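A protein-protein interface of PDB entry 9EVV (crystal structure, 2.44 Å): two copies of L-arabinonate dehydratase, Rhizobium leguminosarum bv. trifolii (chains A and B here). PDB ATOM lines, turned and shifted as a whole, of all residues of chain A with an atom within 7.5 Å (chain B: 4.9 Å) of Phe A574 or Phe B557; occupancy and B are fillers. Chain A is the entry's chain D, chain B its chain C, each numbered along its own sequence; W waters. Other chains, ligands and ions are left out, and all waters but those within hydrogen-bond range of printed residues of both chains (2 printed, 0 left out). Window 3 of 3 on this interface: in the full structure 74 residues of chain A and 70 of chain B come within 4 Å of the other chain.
Water W2 lies within hydrogen-bond range of OE2 of Glu A120 (2.6 Å), OE1 of Glu A119 (2.7 Å) and N of Tyr B555 (2.9 Å). Water W1 lies within hydrogen-bond range of N of Ala B556 (3.1 Å), OE2 of Glu A120 (3.2 Å) and N of Tyr B555 (3.3 Å).
Leu B558 touches its own counterpart, Leu A558. 3 positions are printed for both chains. Of the 9 pairs that touch across the chains among the printed residues, 1 has its exchanged pair printed and touching as well.
Among the printed residues, pairs that only touch across the chains: Phe A574 with Ser B553 (3.1 Å), Glu A120 with Tyr B555 (3.2 Å), Leu A116 with Tyr B555 (3.5 Å), Leu A558 with Leu B558 (3.5 Å), Arg A579 with Gly B554 (3.6 Å), Phe A574 with Phe B557 (3.7 Å) and Leu A575 with Gly B554 (3.9 Å).
Phe A574 touches just these residues of chain B: Ser B553, Gly B554 and Phe B557. Of the printed residues of chain A, Tyr B555 touches Leu A116 and Glu A120. Printed residues of chain B within 4 Å of Leu A558: Leu B558 (3.5 Å). Of the printed residues of chain B, Arg A579 touches Ser B553 and Gly B554. Printed residues of chain B within 4 Å of Leu A575: Gly B554 (3.9 Å). The nearest residue of chain A that does not touch Phe B557 is His A562 (4.7 Å). The nearest printed residue of chain A that does not touch Gly B554 is Glu A119 (5.0 Å).
The guanidinium group (NH1) of Arg A579 lies within hydrogen-bond range of the side-chain hydroxyl (OG) of Ser B553. N of Gly B554 sits at hydrogen-bond distance from O of Phe A574.
Hydrophobic or aromatic side chains of chain A that line the printed part of chain B: Leu A116, Leu A558, Phe A574 and Leu A575. Along chain A the printed residues that touch a printed residue of chain B span positions 116 to 579. Of the 11 printed residues of chain B, 5 touch a printed residue of chain A. Hydrophobic or aromatic side chains of chain B that line the printed part of chain A: Tyr B555, Phe B557 and Leu B558. Among the printed residues, no Asp or Glu carboxylate lies within 4 Å of a Lys or Arg side-chain nitrogen of the other chain.
The side-chain carboxylate (OE2) of Glu A119 lies within salt-bridge range of the guanidinium group (NE) of Arg A579, at 2.6 Å. NE of Arg A298 lies within hydrogen-bond range of O of Leu A575 (3.0 Å). O of Leu A575 sits at hydrogen-bond distance from NH2 of Arg A579. The guanidinium group (NH1) of Arg A579 is in hydrogen-bond range of the backbone carbonyl oxygen (O) of Lys A576 (3.0 Å). O of Gly A577 lies within hydrogen-bond range of NH2 of Arg A579 (3.2 Å).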
ATOM      1  N   LEU A 116       0.535 -15.253  13.498  1.00  0.00           N
ATOM      2  CA  LEU A 116       0.221 -13.877  13.877  1.00  0.00           C
ATOM      3  C   LEU A 116      -0.906 -13.336  13.014  1.00  0.00           C
ATOM      4  O   LEU A 116      -1.941 -12.878  13.522  1.00  0.00           O
ATOM      5  CB  LEU A 116       1.454 -12.980  13.734  1.00  0.00           C
ATOM      6  CG  LEU A 116       1.592 -11.757  14.650  1.00  0.00           C
ATOM      7  CD1 LEU A 116       2.728 -10.909  14.130  1.00  0.00           C
ATOM      8  CD2 LEU A 116       0.307 -10.940  14.781  1.00  0.00           C
ATOM      9  N   GLU A 119      -4.322 -15.045  13.706  1.00  0.00           N
ATOM     10  CA  GLU A 119      -4.952 -14.607  14.953  1.00  0.00           C
ATOM     11  C   GLU A 119      -5.582 -13.224  14.800  1.00  0.00           C
ATOM     12  O   GLU A 119      -6.742 -13.009  15.176  1.00  0.00           O
ATOM     13  CB  GLU A 119      -3.935 -14.601  16.105  1.00  0.00           C
ATOM     14  CG  GLU A 119      -4.439 -13.873  17.385  1.00  0.00           C
ATOM     15  CD  GLU A 119      -3.359 -13.628  18.442  1.00  0.00           C
ATOM     16  OE1 GLU A 119      -2.191 -14.043  18.255  1.00  0.00           O
ATOM     17  OE2 GLU A 119      -3.693 -13.026  19.484  1.00  0.00           O
ATOM     18  N   GLU A 120      -4.825 -12.262  14.270  1.00  0.00           N
ATOM     19  CA  GLU A 120      -5.384 -10.924  14.090  1.00  0.00           C
ATOM     20  C   GLU A 120      -6.575 -10.942  13.127  1.00  0.00           C
ATOM     21  O   GLU A 120      -7.608 -10.316  13.398  1.00  0.00           O
ATOM     22  CB  GLU A 120      -4.294  -9.962  13.620  1.00  0.00           C
ATOM     23  CG  GLU A 120      -3.222  -9.629  14.681  1.00  0.00           C
ATOM     24  CD  GLU A 120      -3.797  -9.299  16.059  1.00  0.00           C
ATOM     25  OE1 GLU A 120      -4.743  -8.493  16.141  1.00  0.00           O
ATOM     26  OE2 GLU A 120      -3.310  -9.841  17.069  1.00  0.00           O
ATOM     27  N   ARG A 298      -0.130 -22.166  22.825  1.00  0.00           N
ATOM     28  CA  ARG A 298      -1.208 -21.227  22.542  1.00  0.00           C
ATOM     29  C   ARG A 298      -2.484 -21.597  23.290  1.00  0.00           C
ATOM     30  O   ARG A 298      -3.137 -20.729  23.870  1.00  0.00           O
ATOM     31  CB  ARG A 298      -1.482 -21.170  21.041  1.00  0.00           C
ATOM     32  CG  ARG A 298      -0.273 -20.825  20.208  1.00  0.00           C
ATOM     33  CD  ARG A 298       0.240 -19.470  20.575  1.00  0.00           C
ATOM     34  NE  ARG A 298       1.152 -18.949  19.567  1.00  0.00           N
ATOM     35  CZ  ARG A 298       0.793 -18.138  18.583  1.00  0.00           C
ATOM     36  NH1 ARG A 298      -0.466 -17.755  18.423  1.00  0.00           N
ATOM     37  NH2 ARG A 298       1.724 -17.688  17.747  1.00  0.00           N
ATOM     38  N   LEU A 558      13.067  -9.168  13.531  1.00  0.00           N
ATOM     39  CA  LEU A 558      12.078  -9.512  14.544  1.00  0.00           C
ATOM     40  C   LEU A 558      12.222 -10.974  14.956  1.00  0.00           C
ATOM     41  O   LEU A 558      12.314 -11.294  16.150  1.00  0.00           O
ATOM     42  CB  LEU A 558      10.678  -9.215  14.001  1.00  0.00           C
ATOM     43  CG  LEU A 558       9.440  -9.701  14.754  1.00  0.00           C
ATOM     44  CD1 LEU A 558       9.134  -8.814  15.932  1.00  0.00           C
ATOM     45  CD2 LEU A 558       8.265  -9.739  13.810  1.00  0.00           C
ATOM     46  N   HIS A 559      12.281 -11.877  13.964  1.00  0.00           N
ATOM     47  CA  HIS A 559      12.477 -13.300  14.243  1.00  0.00           C
ATOM     48  C   HIS A 559      13.741 -13.536  15.074  1.00  0.00           C
ATOM     49  O   HIS A 559      13.706 -14.222  16.104  1.00  0.00           O
ATOM     50  CB  HIS A 559      12.539 -14.076  12.922  1.00  0.00           C
ATOM     51  CG  HIS A 559      12.837 -15.537  13.079  1.00  0.00           C
ATOM     52  ND1 HIS A 559      11.868 -16.466  13.394  1.00  0.00           N
ATOM     53  CD2 HIS A 559      13.997 -16.229  12.955  1.00  0.00           C
ATOM     54  CE1 HIS A 559      12.421 -17.664  13.471  1.00  0.00           C
ATOM     55  NE2 HIS A 559      13.713 -17.548  13.211  1.00  0.00           N
ATOM     56  N   GLN A 561      15.167 -11.766  17.134  1.00  0.00           N
ATOM     57  CA  GLN A 561      15.088 -11.206  18.478  1.00  0.00           C
ATOM     58  C   GLN A 561      14.150 -11.955  19.418  1.00  0.00           C
ATOM     59  O   GLN A 561      14.252 -11.773  20.631  1.00  0.00           O
ATOM     60  CB  GLN A 561      14.646  -9.740  18.395  1.00  0.00           C
ATOM     61  CG  GLN A 561      14.613  -9.009  19.689  1.00  0.00           C
ATOM     62  CD  GLN A 561      15.779  -8.052  19.813  1.00  0.00           C
ATOM     63  OE1 GLN A 561      16.900  -8.367  19.404  1.00  0.00           O
ATOM     64  NE2 GLN A 561      15.520  -6.869  20.353  1.00  0.00           N
ATOM     65  N   HIS A 562      13.251 -12.789  18.900  1.00  0.00           N
ATOM     66  CA  HIS A 562      12.095 -13.252  19.659  1.00  0.00           C
ATOM     67  C   HIS A 562      11.817 -14.739  19.539  1.00  0.00           C
ATOM     68  O   HIS A 562      10.921 -15.230  20.233  1.00  0.00           O
ATOM     69  CB  HIS A 562      10.829 -12.495  19.201  1.00  0.00           C
ATOM     70  CG  HIS A 562      10.765 -11.072  19.668  1.00  0.00           C
ATOM     71  ND1 HIS A 562      10.286 -10.724  20.910  1.00  0.00           N
ATOM     72  CD2 HIS A 562      11.124  -9.915  19.063  1.00  0.00           C
ATOM     73  CE1 HIS A 562      10.345  -9.411  21.051  1.00  0.00           C
ATOM     74  NE2 HIS A 562      10.862  -8.899  19.950  1.00  0.00           N
ATOM     75  N   VAL A 563      12.494 -15.461  18.661  1.00  0.00           N
ATOM     76  CA  VAL A 563      12.176 -16.864  18.463  1.00  0.00           C
ATOM     77  C   VAL A 563      12.810 -17.680  19.583  1.00  0.00           C
ATOM     78  O   VAL A 563      13.996 -17.520  19.897  1.00  0.00           O
ATOM     79  CB  VAL A 563      12.633 -17.336  17.071  1.00  0.00           C
ATOM     80  CG1 VAL A 563      14.157 -17.476  16.993  1.00  0.00           C
ATOM     81  CG2 VAL A 563      11.935 -18.631  16.705  1.00  0.00           C
ATOM     82  N   GLU A 564      12.008 -18.537  20.209  1.00  0.00           N
ATOM     83  CA  GLU A 564      12.478 -19.442  21.242  1.00  0.00           C
ATOM     84  C   GLU A 564      13.058 -20.699  20.602  1.00  0.00           C
ATOM     85  O   GLU A 564      13.028 -20.881  19.381  1.00  0.00           O
ATOM     86  CB  GLU A 564      11.340 -19.778  22.201  1.00  0.00           C
ATOM     87  CG  GLU A 564      10.624 -18.530  22.687  1.00  0.00           C
ATOM     88  CD  GLU A 564       9.786 -18.752  23.927  1.00  0.00           C
ATOM     89  OE1 GLU A 564       9.015 -19.746  23.975  1.00  0.00           O
ATOM     90  OE2 GLU A 564       9.894 -17.911  24.849  1.00  0.00           O
ATOM     91  N   ASP A 571       8.218 -21.000  18.995  1.00  0.00           N
ATOM     92  CA  ASP A 571       7.283 -19.887  18.889  1.00  0.00           C
ATOM     93  C   ASP A 571       8.019 -18.569  19.128  1.00  0.00           C
ATOM     94  O   ASP A 571       9.193 -18.540  19.515  1.00  0.00           O
ATOM     95  CB  ASP A 571       6.137 -20.055  19.893  1.00  0.00           C
ATOM     96  CG  ASP A 571       4.875 -19.275  19.500  1.00  0.00           C
ATOM     97  OD1 ASP A 571       4.959 -18.392  18.607  1.00  0.00           O
ATOM     98  OD2 ASP A 571       3.799 -19.533  20.104  1.00  0.00           O
ATOM     99  N   LEU A 572       7.323 -17.463  18.873  1.00  0.00           N
ATOM    100  CA  LEU A 572       7.796 -16.147  19.275  1.00  0.00           C
ATOM    101  C   LEU A 572       7.337 -15.887  20.706  1.00  0.00           C
ATOM    102  O   LEU A 572       6.183 -16.165  21.043  1.00  0.00           O
ATOM    103  CB  LEU A 572       7.267 -15.075  18.327  1.00  0.00           C
ATOM    104  CG  LEU A 572       7.861 -15.042  16.906  1.00  0.00           C
ATOM    105  CD1 LEU A 572       7.464 -13.757  16.183  1.00  0.00           C
ATOM    106  CD2 LEU A 572       9.370 -15.204  16.923  1.00  0.00           C
ATOM    107  N   ASP A 573       8.242 -15.364  21.546  1.00  0.00           N
ATOM    108  CA  ASP A 573       7.953 -15.242  22.979  1.00  0.00           C
ATOM    109  C   ASP A 573       6.707 -14.401  23.244  1.00  0.00           C
ATOM    110  O   ASP A 573       5.868 -14.771  24.075  1.00  0.00           O
ATOM    111  CB  ASP A 573       9.163 -14.673  23.732  1.00  0.00           C
ATOM    112  CG  ASP A 573       9.694 -13.371  23.130  1.00  0.00           C
ATOM    113  OD1 ASP A 573       9.091 -12.826  22.178  1.00  0.00           O
ATOM    114  OD2 ASP A 573      10.733 -12.877  23.621  1.00  0.00           O
ATOM    115  N   PHE A 574       6.547 -13.280  22.547  1.00  0.00           N
ATOM    116  CA  PHE A 574       5.401 -12.435  22.857  1.00  0.00           C
ATOM    117  C   PHE A 574       4.095 -12.995  22.311  1.00  0.00           C
ATOM    118  O   PHE A 574       3.028 -12.546  22.728  1.00  0.00           O
ATOM    119  CB  PHE A 574       5.626 -11.012  22.336  1.00  0.00           C
ATOM    120  CG  PHE A 574       5.682 -10.914  20.846  1.00  0.00           C
ATOM    121  CD1 PHE A 574       6.872 -11.143  20.165  1.00  0.00           C
ATOM    122  CD2 PHE A 574       4.538 -10.612  20.113  1.00  0.00           C
ATOM    123  CE1 PHE A 574       6.924 -11.058  18.771  1.00  0.00           C
ATOM    124  CE2 PHE A 574       4.583 -10.514  18.720  1.00  0.00           C
ATOM    125  CZ  PHE A 574       5.783 -10.743  18.052  1.00  0.00           C
ATOM    126  N   LEU A 575       4.148 -13.955  21.392  1.00  0.00           N
ATOM    127  CA  LEU A 575       2.955 -14.519  20.782  1.00  0.00           C
ATOM    128  C   LEU A 575       2.403 -15.731  21.524  1.00  0.00           C
ATOM    129  O   LEU A 575       1.438 -16.342  21.058  1.00  0.00           O
ATOM    130  CB  LEU A 575       3.249 -14.903  19.335  1.00  0.00           C
ATOM    131  CG  LEU A 575       3.429 -13.769  18.326  1.00  0.00           C
ATOM    132  CD1 LEU A 575       3.721 -14.381  16.961  1.00  0.00           C
ATOM    133  CD2 LEU A 575       2.200 -12.880  18.266  1.00  0.00           C
ATOM    134  N   LYS A 576       2.970 -16.094  22.657  1.00  0.00           N
ATOM    135  CA  LYS A 576       2.534 -17.294  23.355  1.00  0.00           C
ATOM    136  C   LYS A 576       1.209 -17.072  24.082  1.00  0.00           C
ATOM    137  O   LYS A 576       0.916 -15.983  24.585  1.00  0.00           O
ATOM    138  CB  LYS A 576       3.615 -17.754  24.344  1.00  0.00           C
ATOM    139  CG  LYS A 576       4.828 -18.400  23.660  1.00  0.00           C
ATOM    140  CD  LYS A 576       5.908 -18.862  24.640  1.00  0.00           C
ATOM    141  CE  LYS A 576       6.484 -17.697  25.482  1.00  0.00           C
ATOM    142  NZ  LYS A 576       7.325 -18.164  26.646  1.00  0.00           N
ATOM    143  N   GLY A 577       0.410 -18.125  24.142  1.00  0.00           N
ATOM    144  CA  GLY A 577      -0.786 -18.108  24.951  1.00  0.00           C
ATOM    145  C   GLY A 577      -1.992 -17.623  24.186  1.00  0.00           C
ATOM    146  O   GLY A 577      -1.941 -17.301  22.995  1.00  0.00           O
ATOM    147  N   ARG A 579      -5.162 -15.028  23.757  1.00  0.00           N
ATOM    148  CA  ARG A 579      -5.500 -13.631  24.018  1.00  0.00           C
ATOM    149  C   ARG A 579      -6.997 -13.328  23.940  1.00  0.00           C
ATOM    150  O   ARG A 579      -7.393 -12.188  24.186  1.00  0.00           O
ATOM    151  CB  ARG A 579      -4.738 -12.715  23.052  1.00  0.00           C
ATOM    152  CG  ARG A 579      -3.339 -12.375  23.541  1.00  0.00           C
ATOM    153  CD  ARG A 579      -2.462 -11.861  22.410  1.00  0.00           C
ATOM    154  NE  ARG A 579      -2.054 -12.964  21.561  1.00  0.00           N
ATOM    155  CZ  ARG A 579      -1.198 -13.897  21.944  1.00  0.00           C
ATOM    156  NH1 ARG A 579      -0.578 -13.822  23.112  1.00  0.00           N
ATOM    157  NH2 ARG A 579      -0.954 -14.925  21.135  1.00  0.00           N
ATOM    158  N   PRO B 551      -0.588  -3.484  26.633  1.00  0.00           N
ATOM    159  CA  PRO B 551      -0.679  -4.910  26.290  1.00  0.00           C
ATOM    160  C   PRO B 551       0.649  -5.616  26.495  1.00  0.00           C
ATOM    161  O   PRO B 551       1.710  -5.091  26.150  1.00  0.00           O
ATOM    162  CB  PRO B 551      -1.062  -4.892  24.805  1.00  0.00           C
ATOM    163  CG  PRO B 551      -0.544  -3.565  24.288  1.00  0.00           C
ATOM    164  CD  PRO B 551      -0.230  -2.658  25.465  1.00  0.00           C
ATOM    165  N   THR B 552       0.581  -6.826  27.052  1.00  0.00           N
ATOM    166  CA  THR B 552       1.780  -7.594  27.376  1.00  0.00           C
ATOM    167  C   THR B 552       2.116  -8.674  26.354  1.00  0.00           C
ATOM    168  O   THR B 552       3.170  -9.306  26.479  1.00  0.00           O
ATOM    169  CB  THR B 552       1.651  -8.252  28.761  1.00  0.00           C
ATOM    170  OG1 THR B 552       0.310  -8.715  28.963  1.00  0.00           O
ATOM    171  CG2 THR B 552       2.008  -7.271  29.859  1.00  0.00           C
ATOM    172  N   SER B 553       1.270  -8.915  25.353  1.00  0.00           N
ATOM    173  CA  SER B 553       1.576  -9.968  24.385  1.00  0.00           C
ATOM    174  C   SER B 553       0.828  -9.706  23.078  1.00  0.00           C
ATOM    175  O   SER B 553       0.044  -8.760  22.963  1.00  0.00           O
ATOM    176  CB  SER B 553       1.266 -11.353  24.967  1.00  0.00           C
ATOM    177  OG  SER B 553      -0.120 -11.581  25.112  1.00  0.00           O
ATOM    178  N   GLY B 554       1.120 -10.534  22.074  1.00  0.00           N
ATOM    179  CA  GLY B 554       0.405 -10.500  20.807  1.00  0.00           C
ATOM    180  C   GLY B 554       0.765  -9.298  19.945  1.00  0.00           C
ATOM    181  O   GLY B 554       1.653  -8.492  20.253  1.00  0.00           O
ATOM    182  N   TYR B 555       0.042  -9.184  18.826  1.00  0.00           N
ATOM    183  CA  TYR B 555       0.322  -8.091  17.905  1.00  0.00           C
ATOM    184  C   TYR B 555       0.159  -6.732  18.585  1.00  0.00           C
ATOM    185  O   TYR B 555       0.897  -5.787  18.272  1.00  0.00           O
ATOM    186  CB  TYR B 555      -0.577  -8.176  16.674  1.00  0.00           C
ATOM    187  CG  TYR B 555      -0.323  -7.056  15.681  1.00  0.00           C
ATOM    188  CD1 TYR B 555       0.922  -6.896  15.089  1.00  0.00           C
ATOM    189  CD2 TYR B 555      -1.328  -6.151  15.340  1.00  0.00           C
ATOM    190  CE1 TYR B 555       1.160  -5.872  14.185  1.00  0.00           C
ATOM    191  CE2 TYR B 555      -1.095  -5.128  14.432  1.00  0.00           C
ATOM    192  CZ  TYR B 555       0.151  -4.998  13.861  1.00  0.00           C
ATOM    193  OH  TYR B 555       0.400  -3.987  12.962  1.00  0.00           O
ATOM    194  N   ALA B 556      -0.793  -6.617  19.516  1.00  0.00           N
ATOM    195  CA  ALA B 556      -0.972  -5.360  20.233  1.00  0.00           C
ATOM    196  C   ALA B 556       0.326  -4.955  20.904  1.00  0.00           C
ATOM    197  O   ALA B 556       0.780  -3.818  20.767  1.00  0.00           O
ATOM    198  CB  ALA B 556      -2.104  -5.484  21.250  1.00  0.00           C
ATOM    199  N   PHE B 557       0.966  -5.906  21.581  1.00  0.00           N
ATOM    200  CA  PHE B 557       2.300  -5.687  22.133  1.00  0.00           C
ATOM    201  C   PHE B 557       3.266  -5.170  21.067  1.00  0.00           C
ATOM    202  O   PHE B 557       3.844  -4.083  21.204  1.00  0.00           O
ATOM    203  CB  PHE B 557       2.815  -6.990  22.755  1.00  0.00           C
ATOM    204  CG  PHE B 557       4.220  -6.902  23.257  1.00  0.00           C
ATOM    205  CD1 PHE B 557       4.494  -6.371  24.506  1.00  0.00           C
ATOM    206  CD2 PHE B 557       5.276  -7.330  22.478  1.00  0.00           C
ATOM    207  CE1 PHE B 557       5.801  -6.274  24.965  1.00  0.00           C
ATOM    208  CE2 PHE B 557       6.591  -7.234  22.942  1.00  0.00           C
ATOM    209  CZ  PHE B 557       6.850  -6.707  24.181  1.00  0.00           C
ATOM    210  N   LEU B 558       3.463  -5.948  19.998  1.00  0.00           N
ATOM    211  CA  LEU B 558       4.418  -5.561  18.966  1.00  0.00           C
ATOM    212  C   LEU B 558       4.152  -4.150  18.466  1.00  0.00           C
ATOM    213  O   LEU B 558       5.086  -3.364  18.257  1.00  0.00           O
ATOM    214  CB  LEU B 558       4.356  -6.567  17.822  1.00  0.00           C
ATOM    215  CG  LEU B 558       5.216  -6.288  16.589  1.00  0.00           C
ATOM    216  CD1 LEU B 558       6.674  -6.551  16.924  1.00  0.00           C
ATOM    217  CD2 LEU B 558       4.775  -7.168  15.419  1.00  0.00           C
ATOM    218  N   HIS B 559       2.875  -3.817  18.261  1.00  0.00           N
ATOM    219  CA  HIS B 559       2.495  -2.494  17.793  1.00  0.00           C
ATOM    220  C   HIS B 559       2.806  -1.449  18.843  1.00  0.00           C
ATOM    221  O   HIS B 559       3.469  -0.439  18.566  1.00  0.00           O
ATOM    222  CB  HIS B 559       1.005  -2.487  17.463  1.00  0.00           C
ATOM    223  CG  HIS B 559       0.482  -1.152  17.036  1.00  0.00           C
ATOM    224  ND1 HIS B 559       0.660  -0.659  15.762  1.00  0.00           N
ATOM    225  CD2 HIS B 559      -0.240  -0.219  17.707  1.00  0.00           C
ATOM    226  CE1 HIS B 559       0.086   0.531  15.671  1.00  0.00           C
ATOM    227  NE2 HIS B 559      -0.471   0.819  16.835  1.00  0.00           N
ATOM    228  N   GLN B 560       2.332  -1.683  20.064  1.00  0.00           N
ATOM    229  CA  GLN B 560       2.572  -0.741  21.141  1.00  0.00           C
ATOM    230  C   GLN B 560       4.059  -0.515  21.367  1.00  0.00           C
ATOM    231  O   GLN B 560       4.439   0.567  21.817  1.00  0.00           O
ATOM    232  CB  GLN B 560       1.894  -1.237  22.413  1.00  0.00           C
ATOM    233  CG  GLN B 560       2.046  -0.293  23.589  1.00  0.00           C
ATOM    234  CD  GLN B 560       1.293   1.035  23.410  1.00  0.00           C
ATOM    235  OE1 GLN B 560       1.862   2.092  23.640  1.00  0.00           O
ATOM    236  NE2 GLN B 560       0.018   0.975  23.005  1.00  0.00           N
ATOM    237  N   GLN B 561       4.909  -1.489  21.023  1.00  0.00           N
ATOM    238  CA  GLN B 561       6.350  -1.338  21.212  1.00  0.00           C
ATOM    239  C   GLN B 561       7.054  -0.608  20.083  1.00  0.00           C
ATOM    240  O   GLN B 561       8.073   0.032  20.330  1.00  0.00           O
ATOM    241  CB  GLN B 561       7.027  -2.700  21.358  1.00  0.00           C
ATOM    242  CG  GLN B 561       6.781  -3.398  22.663  1.00  0.00           C
ATOM    243  CD  GLN B 561       7.673  -2.854  23.736  1.00  0.00           C
ATOM    244  OE1 GLN B 561       7.214  -2.175  24.660  1.00  0.00           O
ATOM    245  NE2 GLN B 561       8.968  -3.136  23.619  1.00  0.00           N
HETATM  246  O   HOH W   1      -2.996  -8.673  20.050  1.00  0.00           O
HETATM  247  O   HOH W   2      -1.406 -11.470  17.808  1.00  0.00           O
